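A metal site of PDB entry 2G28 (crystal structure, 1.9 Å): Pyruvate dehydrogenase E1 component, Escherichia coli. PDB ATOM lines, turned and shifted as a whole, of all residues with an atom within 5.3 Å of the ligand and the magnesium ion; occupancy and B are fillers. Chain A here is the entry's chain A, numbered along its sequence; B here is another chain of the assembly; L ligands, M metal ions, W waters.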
ATOM      1  N   HIS A 106      28.745  -1.661 -29.312  1.00  0.00           N
ATOM      2  CA  HIS A 106      27.443  -2.036 -29.859  1.00  0.00           C
ATOM      3  C   HIS A 106      27.448  -2.034 -31.390  1.00  0.00           C
ATOM      4  O   HIS A 106      28.237  -1.338 -32.006  1.00  0.00           O
ATOM      5  CB  HIS A 106      26.351  -1.063 -29.377  1.00  0.00           C
ATOM      6  CG  HIS A 106      26.442  -0.709 -27.926  1.00  0.00           C
ATOM      7  ND1 HIS A 106      25.480  -1.090 -27.008  1.00  0.00           N
ATOM      8  CD2 HIS A 106      27.381  -0.041 -27.232  1.00  0.00           C
ATOM      9  CE1 HIS A 106      25.837  -0.660 -25.801  1.00  0.00           C
ATOM     10  NE2 HIS A 106      26.985  -0.024 -25.918  1.00  0.00           N
ATOM     11  N   SER A 109      22.328  -1.018 -32.734  1.00  0.00           N
ATOM     12  CA  SER A 109      21.723   0.284 -32.740  1.00  0.00           C
ATOM     13  C   SER A 109      22.120   1.138 -33.956  1.00  0.00           C
ATOM     14  O   SER A 109      21.258   1.712 -34.620  1.00  0.00           O
ATOM     15  CB  SER A 109      22.056   1.034 -31.450  1.00  0.00           C
ATOM     16  OG  SER A 109      21.542   2.356 -31.521  1.00  0.00           O
ATOM     17  N   SER A 112      20.465   0.273 -37.127  1.00  0.00           N
ATOM     18  CA  SER A 112      19.104   0.793 -37.272  1.00  0.00           C
ATOM     19  C   SER A 112      19.057   2.270 -37.678  1.00  0.00           C
ATOM     20  O   SER A 112      18.155   2.706 -38.382  1.00  0.00           O
ATOM     21  CB  SER A 112      18.287   0.554 -35.982  1.00  0.00           C
ATOM     22  OG  SER A 112      18.623   1.483 -34.951  1.00  0.00           O
ATOM     23  N   GLN A 140      23.928  10.139 -30.664  1.00  0.00           N
ATOM     24  CA  GLN A 140      23.539   9.147 -29.655  1.00  0.00           C
ATOM     25  C   GLN A 140      24.838   8.420 -29.247  1.00  0.00           C
ATOM     26  O   GLN A 140      25.592   7.926 -30.086  1.00  0.00           O
ATOM     27  CB  GLN A 140      22.493   8.203 -30.227  1.00  0.00           C
ATOM     28  CG  GLN A 140      21.995   7.118 -29.306  1.00  0.00           C
ATOM     29  CD  GLN A 140      20.976   6.225 -29.985  1.00  0.00           C
ATOM     30  OE1 GLN A 140      21.089   5.952 -31.177  1.00  0.00           O
ATOM     31  NE2 GLN A 140      19.984   5.762 -29.230  1.00  0.00           N
ATOM     32  N   HIS A 142      26.008   5.409 -27.915  1.00  0.00           N
ATOM     33  CA  HIS A 142      26.429   4.103 -28.378  1.00  0.00           C
ATOM     34  C   HIS A 142      26.484   3.843 -29.881  1.00  0.00           C
ATOM     35  O   HIS A 142      26.693   2.699 -30.303  1.00  0.00           O
ATOM     36  CB  HIS A 142      25.641   3.003 -27.648  1.00  0.00           C
ATOM     37  CG  HIS A 142      24.146   3.127 -27.756  1.00  0.00           C
ATOM     38  ND1 HIS A 142      23.460   4.262 -27.377  1.00  0.00           N
ATOM     39  CD2 HIS A 142      23.219   2.221 -28.116  1.00  0.00           C
ATOM     40  CE1 HIS A 142      22.157   4.042 -27.499  1.00  0.00           C
ATOM     41  NE2 HIS A 142      21.989   2.805 -27.943  1.00  0.00           N
ATOM     42  N   TYR A 177      32.513   6.163 -25.887  1.00  0.00           N
ATOM     43  CA  TYR A 177      31.453   7.123 -26.215  1.00  0.00           C
ATOM     44  C   TYR A 177      31.947   8.565 -26.359  1.00  0.00           C
ATOM     45  O   TYR A 177      33.113   8.853 -26.157  1.00  0.00           O
ATOM     46  CB  TYR A 177      30.396   7.036 -25.126  1.00  0.00           C
ATOM     47  CG  TYR A 177      29.959   5.619 -24.806  1.00  0.00           C
ATOM     48  CD1 TYR A 177      29.295   4.842 -25.763  1.00  0.00           C
ATOM     49  CD2 TYR A 177      30.195   5.062 -23.549  1.00  0.00           C
ATOM     50  CE1 TYR A 177      28.875   3.555 -25.474  1.00  0.00           C
ATOM     51  CE2 TYR A 177      29.781   3.754 -23.258  1.00  0.00           C
ATOM     52  CZ  TYR A 177      29.116   3.013 -24.226  1.00  0.00           C
ATOM     53  OH  TYR A 177      28.679   1.739 -23.948  1.00  0.00           O
ATOM     54  N   VAL A 192      25.999   9.691 -23.618  1.00  0.00           N
ATOM     55  CA  VAL A 192      25.667   8.344 -23.205  1.00  0.00           C
ATOM     56  C   VAL A 192      24.934   8.200 -21.895  1.00  0.00           C
ATOM     57  O   VAL A 192      24.421   7.127 -21.598  1.00  0.00           O
ATOM     58  CB  VAL A 192      26.881   7.448 -23.169  1.00  0.00           C
ATOM     59  CG1 VAL A 192      26.476   6.053 -23.579  1.00  0.00           C
ATOM     60  CG2 VAL A 192      27.888   7.972 -24.091  1.00  0.00           C
ATOM     61  N   SER A 193      24.891   9.263 -21.104  1.00  0.00           N
ATOM     62  CA  SER A 193      24.085   9.177 -19.881  1.00  0.00           C
ATOM     63  C   SER A 193      22.742   9.663 -20.397  1.00  0.00           C
ATOM     64  O   SER A 193      22.538  10.864 -20.546  1.00  0.00           O
ATOM     65  CB  SER A 193      24.558  10.125 -18.787  1.00  0.00           C
ATOM     66  OG  SER A 193      23.687  10.019 -17.668  1.00  0.00           O
ATOM     67  N   MET A 194      21.860   8.713 -20.687  1.00  0.00           N
ATOM     68  CA  MET A 194      20.535   8.963 -21.255  1.00  0.00           C
ATOM     69  C   MET A 194      19.752  10.061 -20.587  1.00  0.00           C
ATOM     70  O   MET A 194      19.736  10.171 -19.366  1.00  0.00           O
ATOM     71  CB  MET A 194      19.695   7.690 -21.206  1.00  0.00           C
ATOM     72  CG  MET A 194      20.466   6.415 -21.419  1.00  0.00           C
ATOM     73  SD  MET A 194      20.196   5.711 -23.026  1.00  0.00           S
ATOM     74  CE  MET A 194      21.023   7.078 -23.955  1.00  0.00           C
ATOM     75  N   GLY A 229      17.163   7.941 -28.387  1.00  0.00           N
ATOM     76  CA  GLY A 229      16.621   6.603 -28.540  1.00  0.00           C
ATOM     77  C   GLY A 229      15.183   6.655 -28.028  1.00  0.00           C
ATOM     78  O   GLY A 229      14.847   7.544 -27.253  1.00  0.00           O
ATOM     79  N   ASP A 230      14.322   5.718 -28.437  1.00  0.00           N
ATOM     80  CA  ASP A 230      12.962   5.756 -27.928  1.00  0.00           C
ATOM     81  C   ASP A 230      12.909   5.266 -26.472  1.00  0.00           C
ATOM     82  O   ASP A 230      12.123   5.768 -25.661  1.00  0.00           O
ATOM     83  CB  ASP A 230      11.991   4.982 -28.837  1.00  0.00           C
ATOM     84  CG  ASP A 230      12.487   3.592 -29.257  1.00  0.00           C
ATOM     85  OD1 ASP A 230      13.621   3.189 -28.921  1.00  0.00           O
ATOM     86  OD2 ASP A 230      11.707   2.908 -29.965  1.00  0.00           O
ATOM     87  N   GLY A 231      13.768   4.317 -26.125  1.00  0.00           N
ATOM     88  CA  GLY A 231      13.814   3.842 -24.751  1.00  0.00           C
ATOM     89  C   GLY A 231      14.273   4.982 -23.836  1.00  0.00           C
ATOM     90  O   GLY A 231      13.789   5.140 -22.722  1.00  0.00           O
ATOM     91  N   GLU A 232      15.199   5.785 -24.338  1.00  0.00           N
ATOM     92  CA  GLU A 232      15.741   6.927 -23.616  1.00  0.00           C
ATOM     93  C   GLU A 232      14.693   7.985 -23.270  1.00  0.00           C
ATOM     94  O   GLU A 232      14.843   8.728 -22.292  1.00  0.00           O
ATOM     95  CB  GLU A 232      16.874   7.550 -24.432  1.00  0.00           C
ATOM     96  CG  GLU A 232      17.220   8.981 -24.076  1.00  0.00           C
ATOM     97  CD  GLU A 232      18.482   9.450 -24.795  1.00  0.00           C
ATOM     98  OE1 GLU A 232      18.718   8.975 -25.935  1.00  0.00           O
ATOM     99  OE2 GLU A 232      19.218  10.303 -24.238  1.00  0.00           O
ATOM    100  N   GLU A 235      13.329   8.629 -19.646  1.00  0.00           N
ATOM    101  CA  GLU A 235      14.029   9.395 -18.594  1.00  0.00           C
ATOM    102  C   GLU A 235      13.231  10.672 -18.392  1.00  0.00           C
ATOM    103  O   GLU A 235      12.910  11.361 -19.355  1.00  0.00           O
ATOM    104  CB  GLU A 235      15.464   9.744 -19.005  1.00  0.00           C
ATOM    105  CG  GLU A 235      16.427   8.551 -19.054  1.00  0.00           C
ATOM    106  CD  GLU A 235      16.799   8.014 -17.677  1.00  0.00           C
ATOM    107  OE1 GLU A 235      16.154   8.395 -16.682  1.00  0.00           O
ATOM    108  OE2 GLU A 235      17.737   7.204 -17.611  1.00  0.00           O
ATOM    109  N   ASN A 258      15.006   7.770 -32.601  1.00  0.00           N
ATOM    110  CA  ASN A 258      15.098   6.516 -33.329  1.00  0.00           C
ATOM    111  C   ASN A 258      14.094   5.539 -32.717  1.00  0.00           C
ATOM    112  O   ASN A 258      14.321   4.948 -31.661  1.00  0.00           O
ATOM    113  CB  ASN A 258      16.514   5.955 -33.265  1.00  0.00           C
ATOM    114  CG  ASN A 258      16.643   4.665 -34.032  1.00  0.00           C
ATOM    115  OD1 ASN A 258      15.711   4.293 -34.721  1.00  0.00           O
ATOM    116  ND2 ASN A 258      17.777   3.988 -33.913  1.00  0.00           N
ATOM    117  N   ASN A 260      12.952   2.327 -32.907  1.00  0.00           N
ATOM    118  CA  ASN A 260      13.111   0.937 -33.334  1.00  0.00           C
ATOM    119  C   ASN A 260      12.223   0.080 -32.413  1.00  0.00           C
ATOM    120  O   ASN A 260      12.222  -1.139 -32.491  1.00  0.00           O
ATOM    121  CB  ASN A 260      14.590   0.497 -33.268  1.00  0.00           C
ATOM    122  CG  ASN A 260      15.281   0.936 -31.992  1.00  0.00           C
ATOM    123  OD1 ASN A 260      14.648   1.112 -30.957  1.00  0.00           O
ATOM    124  ND2 ASN A 260      16.602   1.110 -32.062  1.00  0.00           N
ATOM    125  N   LEU A 261      11.466   0.773 -31.563  1.00  0.00           N
ATOM    126  CA  LEU A 261      10.507   0.167 -30.642  1.00  0.00           C
ATOM    127  C   LEU A 261      11.145  -0.705 -29.554  1.00  0.00           C
ATOM    128  O   LEU A 261      10.407  -1.353 -28.796  1.00  0.00           O
ATOM    129  CB  LEU A 261       9.480  -0.692 -31.386  1.00  0.00           C
ATOM    130  CG  LEU A 261       8.842  -0.103 -32.635  1.00  0.00           C
ATOM    131  CD1 LEU A 261       7.900  -1.137 -33.235  1.00  0.00           C
ATOM    132  CD2 LEU A 261       8.107   1.186 -32.309  1.00  0.00           C
ATOM    133  N   GLN A 262      12.475  -0.719 -29.488  1.00  0.00           N
ATOM    134  CA  GLN A 262      13.179  -1.542 -28.491  1.00  0.00           C
ATOM    135  C   GLN A 262      14.145  -0.754 -27.621  1.00  0.00           C
ATOM    136  O   GLN A 262      14.690   0.278 -28.035  1.00  0.00           O
ATOM    137  CB  GLN A 262      14.017  -2.655 -29.164  1.00  0.00           C
ATOM    138  CG  GLN A 262      13.399  -3.358 -30.377  1.00  0.00           C
ATOM    139  CD  GLN A 262      14.275  -4.511 -30.932  1.00  0.00           C
ATOM    140  OE1 GLN A 262      14.040  -5.000 -32.040  1.00  0.00           O
ATOM    141  NE2 GLN A 262      15.282  -4.948 -30.147  1.00  0.00           N
ATOM    142  N   ARG A 263      14.347  -1.248 -26.397  1.00  0.00           N
ATOM    143  CA  ARG A 263      15.350  -0.676 -25.512  1.00  0.00           C
ATOM    144  C   ARG A 263      16.332  -1.826 -25.295  1.00  0.00           C
ATOM    145  O   ARG A 263      16.593  -2.608 -26.230  1.00  0.00           O
ATOM    146  CB  ARG A 263      14.777  -0.132 -24.187  1.00  0.00           C
ATOM    147  CG  ARG A 263      13.586  -0.842 -23.556  1.00  0.00           C
ATOM    148  CD  ARG A 263      13.281  -0.137 -22.209  1.00  0.00           C
ATOM    149  NE  ARG A 263      11.999  -0.536 -21.629  1.00  0.00           N
ATOM    150  CZ  ARG A 263      11.699  -1.764 -21.212  1.00  0.00           C
ATOM    151  NH1 ARG A 263      12.593  -2.752 -21.311  1.00  0.00           N
ATOM    152  NH2 ARG A 263      10.492  -2.022 -20.740  1.00  0.00           N
ATOM    153  N   LEU A 264      16.886  -1.974 -24.101  1.00  0.00           N
ATOM    154  CA  LEU A 264      17.828  -3.065 -23.904  1.00  0.00           C
ATOM    155  C   LEU A 264      17.202  -4.426 -23.600  1.00  0.00           C
ATOM    156  O   LEU A 264      17.530  -5.434 -24.253  1.00  0.00           O
ATOM    157  CB  LEU A 264      18.814  -2.680 -22.803  1.00  0.00           C
ATOM    158  CG  LEU A 264      20.215  -3.282 -22.836  1.00  0.00           C
ATOM    159  CD1 LEU A 264      20.155  -4.756 -22.488  1.00  0.00           C
ATOM    160  CD2 LEU A 264      20.843  -3.048 -24.208  1.00  0.00           C
ATOM    161  N   VAL A 268      10.035  -0.971 -25.751  1.00  0.00           N
ATOM    162  CA  VAL A 268       9.762   0.142 -24.848  1.00  0.00           C
ATOM    163  C   VAL A 268       8.400  -0.088 -24.189  1.00  0.00           C
ATOM    164  O   VAL A 268       8.282  -0.052 -22.962  1.00  0.00           O
ATOM    165  CB  VAL A 268       9.767   1.496 -25.610  1.00  0.00           C
ATOM    166  CG1 VAL A 268       9.633   2.654 -24.625  1.00  0.00           C
ATOM    167  CG2 VAL A 268      11.071   1.648 -26.417  1.00  0.00           C
ATOM    168  N   LYS A 392      15.898  -2.456 -35.213  1.00  0.00           N
ATOM    169  CA  LYS A 392      17.125  -2.634 -34.422  1.00  0.00           C
ATOM    170  C   LYS A 392      17.848  -3.877 -34.910  1.00  0.00           C
ATOM    171  O   LYS A 392      17.241  -4.924 -35.053  1.00  0.00           O
ATOM    172  CB  LYS A 392      16.779  -2.792 -32.939  1.00  0.00           C
ATOM    173  CG  LYS A 392      17.981  -2.917 -32.006  1.00  0.00           C
ATOM    174  CD  LYS A 392      17.547  -2.490 -30.596  1.00  0.00           C
ATOM    175  CE  LYS A 392      18.668  -2.572 -29.559  1.00  0.00           C
ATOM    176  NZ  LYS A 392      18.297  -1.673 -28.381  1.00  0.00           N
ATOM    177  N   ALA B 520      15.964  -1.054 -14.044  1.00  0.00           N
ATOM    178  CA  ALA B 520      15.734   0.046 -14.975  1.00  0.00           C
ATOM    179  C   ALA B 520      16.270  -0.407 -16.323  1.00  0.00           C
ATOM    180  O   ALA B 520      17.387  -0.073 -16.697  1.00  0.00           O
ATOM    181  CB  ALA B 520      16.433   1.321 -14.500  1.00  0.00           C
ATOM    182  N   ASP B 521      15.422  -1.182 -17.000  1.00  0.00           N
ATOM    183  CA  ASP B 521      15.656  -1.769 -18.301  1.00  0.00           C
ATOM    184  C   ASP B 521      16.586  -2.949 -18.128  1.00  0.00           C
ATOM    185  O   ASP B 521      16.174  -4.128 -18.282  1.00  0.00           O
ATOM    186  CB  ASP B 521      16.234  -0.753 -19.312  1.00  0.00           C
ATOM    187  CG  ASP B 521      16.216  -1.261 -20.765  1.00  0.00           C
ATOM    188  OD1 ASP B 521      15.532  -2.274 -21.046  1.00  0.00           O
ATOM    189  OD2 ASP B 521      16.855  -0.651 -21.642  1.00  0.00           O
ATOM    190  N   GLU B 522      17.811  -2.656 -17.723  1.00  0.00           N
ATOM    191  CA  GLU B 522      18.850  -3.651 -17.568  1.00  0.00           C
ATOM    192  C   GLU B 522      18.709  -4.824 -16.598  1.00  0.00           C
ATOM    193  O   GLU B 522      18.873  -4.710 -15.382  1.00  0.00           O
ATOM    194  CB  GLU B 522      20.175  -2.942 -17.349  1.00  0.00           C
ATOM    195  CG  GLU B 522      20.900  -2.720 -18.697  1.00  0.00           C
ATOM    196  CD  GLU B 522      19.990  -2.139 -19.802  1.00  0.00           C
ATOM    197  OE1 GLU B 522      18.735  -2.336 -19.744  1.00  0.00           O
ATOM    198  OE2 GLU B 522      20.550  -1.503 -20.740  1.00  0.00           O
ATOM    199  N   THR B 525      22.032  -7.525 -18.310  1.00  0.00           N
ATOM    200  CA  THR B 525      23.372  -7.161 -17.872  1.00  0.00           C
ATOM    201  C   THR B 525      23.701  -7.754 -16.496  1.00  0.00           C
ATOM    202  O   THR B 525      24.866  -8.047 -16.193  1.00  0.00           O
ATOM    203  CB  THR B 525      23.551  -5.632 -17.788  1.00  0.00           C
ATOM    204  OG1 THR B 525      23.304  -5.040 -19.086  1.00  0.00           O
ATOM    205  CG2 THR B 525      24.967  -5.282 -17.329  1.00  0.00           C
ATOM    206  N   ILE B 569      14.281   2.664 -18.949  1.00  0.00           N
ATOM    207  CA  ILE B 569      15.423   3.551 -18.786  1.00  0.00           C
ATOM    208  C   ILE B 569      14.893   4.775 -18.034  1.00  0.00           C
ATOM    209  O   ILE B 569      14.643   5.840 -18.606  1.00  0.00           O
ATOM    210  CB  ILE B 569      15.984   3.944 -20.168  1.00  0.00           C
ATOM    211  CG1 ILE B 569      16.112   2.664 -21.022  1.00  0.00           C
ATOM    212  CG2 ILE B 569      17.347   4.633 -20.005  1.00  0.00           C
ATOM    213  CD1 ILE B 569      16.827   2.867 -22.350  1.00  0.00           C
ATOM    214  N   GLU B 571      15.815   5.854 -14.126  1.00  0.00           N
ATOM    215  CA  GLU B 571      16.326   5.646 -12.777  1.00  0.00           C
ATOM    216  C   GLU B 571      15.471   6.330 -11.718  1.00  0.00           C
ATOM    217  O   GLU B 571      15.221   5.758 -10.661  1.00  0.00           O
ATOM    218  CB  GLU B 571      17.778   6.098 -12.650  1.00  0.00           C
ATOM    219  CG  GLU B 571      18.787   5.147 -13.295  1.00  0.00           C
ATOM    220  CD  GLU B 571      18.922   5.351 -14.801  1.00  0.00           C
ATOM    221  OE1 GLU B 571      18.437   6.382 -15.298  1.00  0.00           O
ATOM    222  OE2 GLU B 571      19.533   4.484 -15.491  1.00  0.00           O
ATOM    223  N   TYR B 599      23.006   0.351 -12.702  1.00  0.00           N
ATOM    224  CA  TYR B 599      24.422   0.711 -12.885  1.00  0.00           C
ATOM    225  C   TYR B 599      24.728   1.752 -11.816  1.00  0.00           C
ATOM    226  O   TYR B 599      24.153   2.844 -11.825  1.00  0.00           O
ATOM    227  CB  TYR B 599      24.664   1.322 -14.255  1.00  0.00           C
ATOM    228  CG  TYR B 599      24.482   0.382 -15.433  1.00  0.00           C
ATOM    229  CD1 TYR B 599      24.120  -0.938 -15.247  1.00  0.00           C
ATOM    230  CD2 TYR B 599      24.636   0.855 -16.733  1.00  0.00           C
ATOM    231  CE1 TYR B 599      23.894  -1.773 -16.338  1.00  0.00           C
ATOM    232  CE2 TYR B 599      24.419   0.030 -17.824  1.00  0.00           C
ATOM    233  CZ  TYR B 599      24.036  -1.275 -17.624  1.00  0.00           C
ATOM    234  OH  TYR B 599      23.802  -2.085 -18.726  1.00  0.00           O
ATOM    235  N   PHE B 602      24.673   5.676 -12.060  1.00  0.00           N
ATOM    236  CA  PHE B 602      23.387   6.342 -12.154  1.00  0.00           C
ATOM    237  C   PHE B 602      22.511   6.220 -10.903  1.00  0.00           C
ATOM    238  O   PHE B 602      21.295   6.281 -10.989  1.00  0.00           O
ATOM    239  CB  PHE B 602      22.630   5.828 -13.382  1.00  0.00           C
ATOM    240  CG  PHE B 602      23.451   5.841 -14.636  1.00  0.00           C
ATOM    241  CD1 PHE B 602      24.108   6.983 -15.037  1.00  0.00           C
ATOM    242  CD2 PHE B 602      23.580   4.702 -15.409  1.00  0.00           C
ATOM    243  CE1 PHE B 602      24.887   7.000 -16.193  1.00  0.00           C
ATOM    244  CE2 PHE B 602      24.354   4.705 -16.556  1.00  0.00           C
ATOM    245  CZ  PHE B 602      25.010   5.856 -16.954  1.00  0.00           C
ATOM    246  N   ARG B 606      22.736  10.552  -9.926  1.00  0.00           N
ATOM    247  CA  ARG B 606      21.618  10.923 -10.788  1.00  0.00           C
ATOM    248  C   ARG B 606      20.295  11.126 -10.081  1.00  0.00           C
ATOM    249  O   ARG B 606      19.474  11.922 -10.528  1.00  0.00           O
ATOM    250  CB  ARG B 606      21.476   9.845 -11.870  1.00  0.00           C
ATOM    251  CG  ARG B 606      20.316  10.046 -12.829  1.00  0.00           C
ATOM    252  CD  ARG B 606      20.511  11.238 -13.724  1.00  0.00           C
ATOM    253  NE  ARG B 606      19.507  11.266 -14.794  1.00  0.00           N
ATOM    254  CZ  ARG B 606      19.738  10.966 -16.065  1.00  0.00           C
ATOM    255  NH1 ARG B 606      20.946  10.607 -16.482  1.00  0.00           N
ATOM    256  NH2 ARG B 606      18.744  11.020 -16.938  1.00  0.00           N
ATOM    257  N   GLU B 636      33.500   0.645 -20.569  1.00  0.00           N
ATOM    258  CA  GLU B 636      32.497   1.711 -20.648  1.00  0.00           C
ATOM    259  C   GLU B 636      32.964   3.161 -20.584  1.00  0.00           C
ATOM    260  O   GLU B 636      32.327   4.033 -21.174  1.00  0.00           O
ATOM    261  CB  GLU B 636      31.403   1.429 -19.619  1.00  0.00           C
ATOM    262  CG  GLU B 636      30.699   0.092 -19.864  1.00  0.00           C
ATOM    263  CD  GLU B 636      30.131   0.006 -21.265  1.00  0.00           C
ATOM    264  OE1 GLU B 636      29.508   0.998 -21.684  1.00  0.00           O
ATOM    265  OE2 GLU B 636      30.317  -1.018 -21.933  1.00  0.00           O
ATOM    266  N   HIS B 640      30.414   6.018 -17.124  1.00  0.00           N
ATOM    267  CA  HIS B 640      29.916   4.778 -16.538  1.00  0.00           C
ATOM    268  C   HIS B 640      30.786   4.271 -15.381  1.00  0.00           C
ATOM    269  O   HIS B 640      30.270   3.637 -14.472  1.00  0.00           O
ATOM    270  CB  HIS B 640      29.863   3.649 -17.550  1.00  0.00           C
ATOM    271  CG  HIS B 640      28.771   3.762 -18.577  1.00  0.00           C
ATOM    272  ND1 HIS B 640      28.811   4.656 -19.621  1.00  0.00           N
ATOM    273  CD2 HIS B 640      27.648   3.031 -18.752  1.00  0.00           C
ATOM    274  CE1 HIS B 640      27.767   4.471 -20.405  1.00  0.00           C
ATOM    275  NE2 HIS B 640      27.039   3.488 -19.898  1.00  0.00           N
HETATM  276  O1  LIG L   1      18.591   2.900 -30.343  1.00  0.00           O
HETATM  277  P1  LIG L   1      18.546   2.148 -29.045  1.00  0.00           P
HETATM  278  O2  LIG L   1      19.698   1.312 -28.658  1.00  0.00           O
HETATM  279  O3  LIG L   1      17.207   1.267 -28.999  1.00  0.00           O
HETATM  280  O4  LIG L   1      18.314   3.254 -27.878  1.00  0.00           O
HETATM  281  P2  LIG L   1      17.188   3.128 -26.728  1.00  0.00           P
HETATM  282  O5  LIG L   1      15.933   2.602 -27.289  1.00  0.00           O
HETATM  283  O6  LIG L   1      17.158   4.433 -26.009  1.00  0.00           O
HETATM  284  O7  LIG L   1      17.822   2.039 -25.746  1.00  0.00           O
HETATM  285  C1  LIG L   1      18.951   2.390 -24.964  1.00  0.00           C
HETATM  286  C2  LIG L   1      19.391   1.248 -24.168  1.00  0.00           C
HETATM  287  C3  LIG L   1      20.566   1.528 -23.327  1.00  0.00           C
HETATM  288  S1  LIG L   1      22.099   1.629 -24.065  1.00  0.00           S
HETATM  289  C4  LIG L   1      20.682   1.695 -21.972  1.00  0.00           C
HETATM  290  C5  LIG L   1      19.563   1.656 -21.000  1.00  0.00           C
HETATM  291  N1  LIG L   1      21.979   1.888 -21.573  1.00  0.00           N
HETATM  292  C6  LIG L   1      22.882   1.870 -22.577  1.00  0.00           C
HETATM  293  C7  LIG L   1      24.375   1.703 -22.469  1.00  0.00           C
HETATM  294  O8  LIG L   1      24.873   2.409 -21.319  1.00  0.00           O
HETATM  295  C8  LIG L   1      25.052   2.148 -23.735  1.00  0.00           C
HETATM  296  P3  LIG L   1      24.619  -0.110 -22.213  1.00  0.00           P
HETATM  297  O9  LIG L   1      23.952  -0.518 -20.928  1.00  0.00           O
HETATM  298  O10 LIG L   1      26.205  -0.161 -22.083  1.00  0.00           O
HETATM  299  C9  LIG L   1      26.884  -0.388 -20.911  1.00  0.00           C
HETATM  300  O11 LIG L   1      24.226  -0.851 -23.452  1.00  0.00           O
HETATM  301  C10 LIG L   1      22.369   1.994 -20.114  1.00  0.00           C
HETATM  302  C11 LIG L   1      21.993   3.316 -19.483  1.00  0.00           C
HETATM  303  C12 LIG L   1      21.146   3.380 -18.476  1.00  0.00           C
HETATM  304  N2  LIG L   1      20.849   4.534 -17.866  1.00  0.00           N
HETATM  305  C13 LIG L   1      21.407   5.681 -18.270  1.00  0.00           C
HETATM  306  C14 LIG L   1      21.048   6.927 -17.604  1.00  0.00           C
HETATM  307  N3  LIG L   1      22.267   5.732 -19.267  1.00  0.00           N
HETATM  308  C15 LIG L   1      22.598   4.578 -19.902  1.00  0.00           C
HETATM  309  N4  LIG L   1      23.492   4.665 -20.844  1.00  0.00           N
HETATM  310 MG    MG M   1      15.320   1.896 -29.048  1.00  0.00          MG
HETATM  311  O   HOH W   1      20.376   4.146 -32.922  1.00  0.00           O
HETATM  312  O   HOH W   2      16.027   3.636 -30.234  1.00  0.00           O
HETATM  313  O   HOH W   3      18.526   2.760 -17.256  1.00  0.00           O
HETATM  314  O   HOH W   4      19.318   6.244 -26.664  1.00  0.00           O
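The side-chain hydroxyl (OH) of Tyr 599 of chain B is in hydrogen-bond range of an oxygen (O9) of the ligand, 2.7 Å away. The side-chain carboxylate of Glu 571 of chain B sits at hydrogen-bond distance from a nitrogen (N2) of the ligand. A nitrogen (N4) of the ligand lies within hydrogen-bond range of the backbone carbonyl oxygen of Val 192, at 2.7 Å. A ring nitrogen (NE2) of His 640 of chain B sits at hydrogen-bond distance from an oxygen (O8) of the ligand. O2 of the ligand lies within hydrogen-bond range of NE2 of His 142 (2.8 Å). The backbone NH of Met 194 sits close to a nitrogen (N3) of the ligand (3.3 Å). The backbone NH (N) of Glu 232 lies within hydrogen-bond range of an oxygen (O6) of the ligand. The backbone NH of Gly 231 lies within hydrogen-bond range of an oxygen (O6) of the ligand, at 3.4 Å. The side-chain amino group (NZ) of Lys 392 is in salt-bridge range of an oxygen (O2) of the ligand (3.3 Å). The side-chain hydroxyl (OG) of Ser 109 is in hydrogen-bond range of an oxygen (O1) of the ligand (3.2 Å). The side-chain amide nitrogen of Gln 140 sits at hydrogen-bond distance from an oxygen (O4) of the ligand.
OD2 of Asp 230 lies within hydrogen-bond range of N of Leu 261, 2.7 Å away. The side-chain carboxylate (OE2) of Glu 235 sits close to the side-chain carboxylate (OE1) of Glu 571 of chain B, at 2.6 Å. OH of Tyr 177 lies within hydrogen-bond range of NE2 of His 106, 3.1 Å away. N of Gly 229 lies within hydrogen-bond range of OE1 of Glu 232. N of Glu 235 lies close to O of Ile 569 of chain B, at 3.3 Å. OE1 of Glu 235 is in salt-bridge range of NH2 of Arg 606 of chain B (3.7 Å). The side-chain amide nitrogen (ND2) of Asn 258 is in hydrogen-bond range of the side-chain hydroxyl (OG) of Ser 112. The guanidinium group (NH1) of Arg 606 of chain B is in hydrogen-bond range of the side-chain hydroxyl (OG) of Ser 193.
The magnesium ion is bound by O3 of the ligand (2.0 Å), O5 of the ligand (2.0 Å), O of Gln 262 (2.0 Å), OD1 of Asp 230 (2.1 Å), OD1 of Asn 260 (2.2 Å) and water W2 (2.2 Å).
Water W2 lies within hydrogen-bond range of the backbone carbonyl oxygen of Asn 258 (2.6 Å), an oxygen (O1) of the ligand (2.7 Å), the side-chain amide nitrogen of Asn 260 (3.2 Å) and the backbone NH of Asp 230 (3.2 Å). Water W4 lies within hydrogen-bond range of the side-chain amide nitrogen of Gln 140 (2.7 Å), the side-chain carboxylate of Glu 232 (2.9 Å), an oxygen (O6) of the ligand (2.9 Å), the backbone NH of Gly 229 (3.2 Å) and the side-chain sulfur of Met 194 (3.8 Å). Water W1 lies within hydrogen-bond range of the side-chain hydroxyl (OG) of Ser 109 (2.6 Å), the side-chain amide oxygen (OE1) of Gln 140 (2.6 Å), the side-chain amide nitrogen (ND2) of Asn 258 (2.8 Å) and an oxygen (O1) of the ligand (3.4 Å).
His 106 touches the ligand. Tyr 177 touches the ligand (OH to O10, 3.6 Å). CA of Ser 193 touches N3 of the ligand (3.9 Å). Gly 229 touches the ligand (CA to O6, 3.4 Å). Glu 235 touches the ligand (OE2 to C14, 3.3 Å). Asn 258 touches the ligand. Arg 263 touches the ligand. OD2 of Asp 521 of chain B touches C5 of the ligand, 3.6 Å away. Glu 522 of chain B touches the ligand. Ile 569 of chain B touches the ligand (CD1 to C5, 3.3 Å). Phe 602 of chain B touches the ligand (CE2 to C13, 3.5 Å). Arg 606 of chain B touches the ligand. Glu 636 of chain B touches the ligand (OE1 to C9, 3.1 Å). Hydrophobic or aromatic side chains that line the ligand: His 106, His 142, Met 194, Ile 569 of chain B, Tyr 599 of chain B, Phe 602 of chain B and His 640 of chain B.
The nearest printed residue that does not touch the magnesium ion is Gly 231 (4.1 Å).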
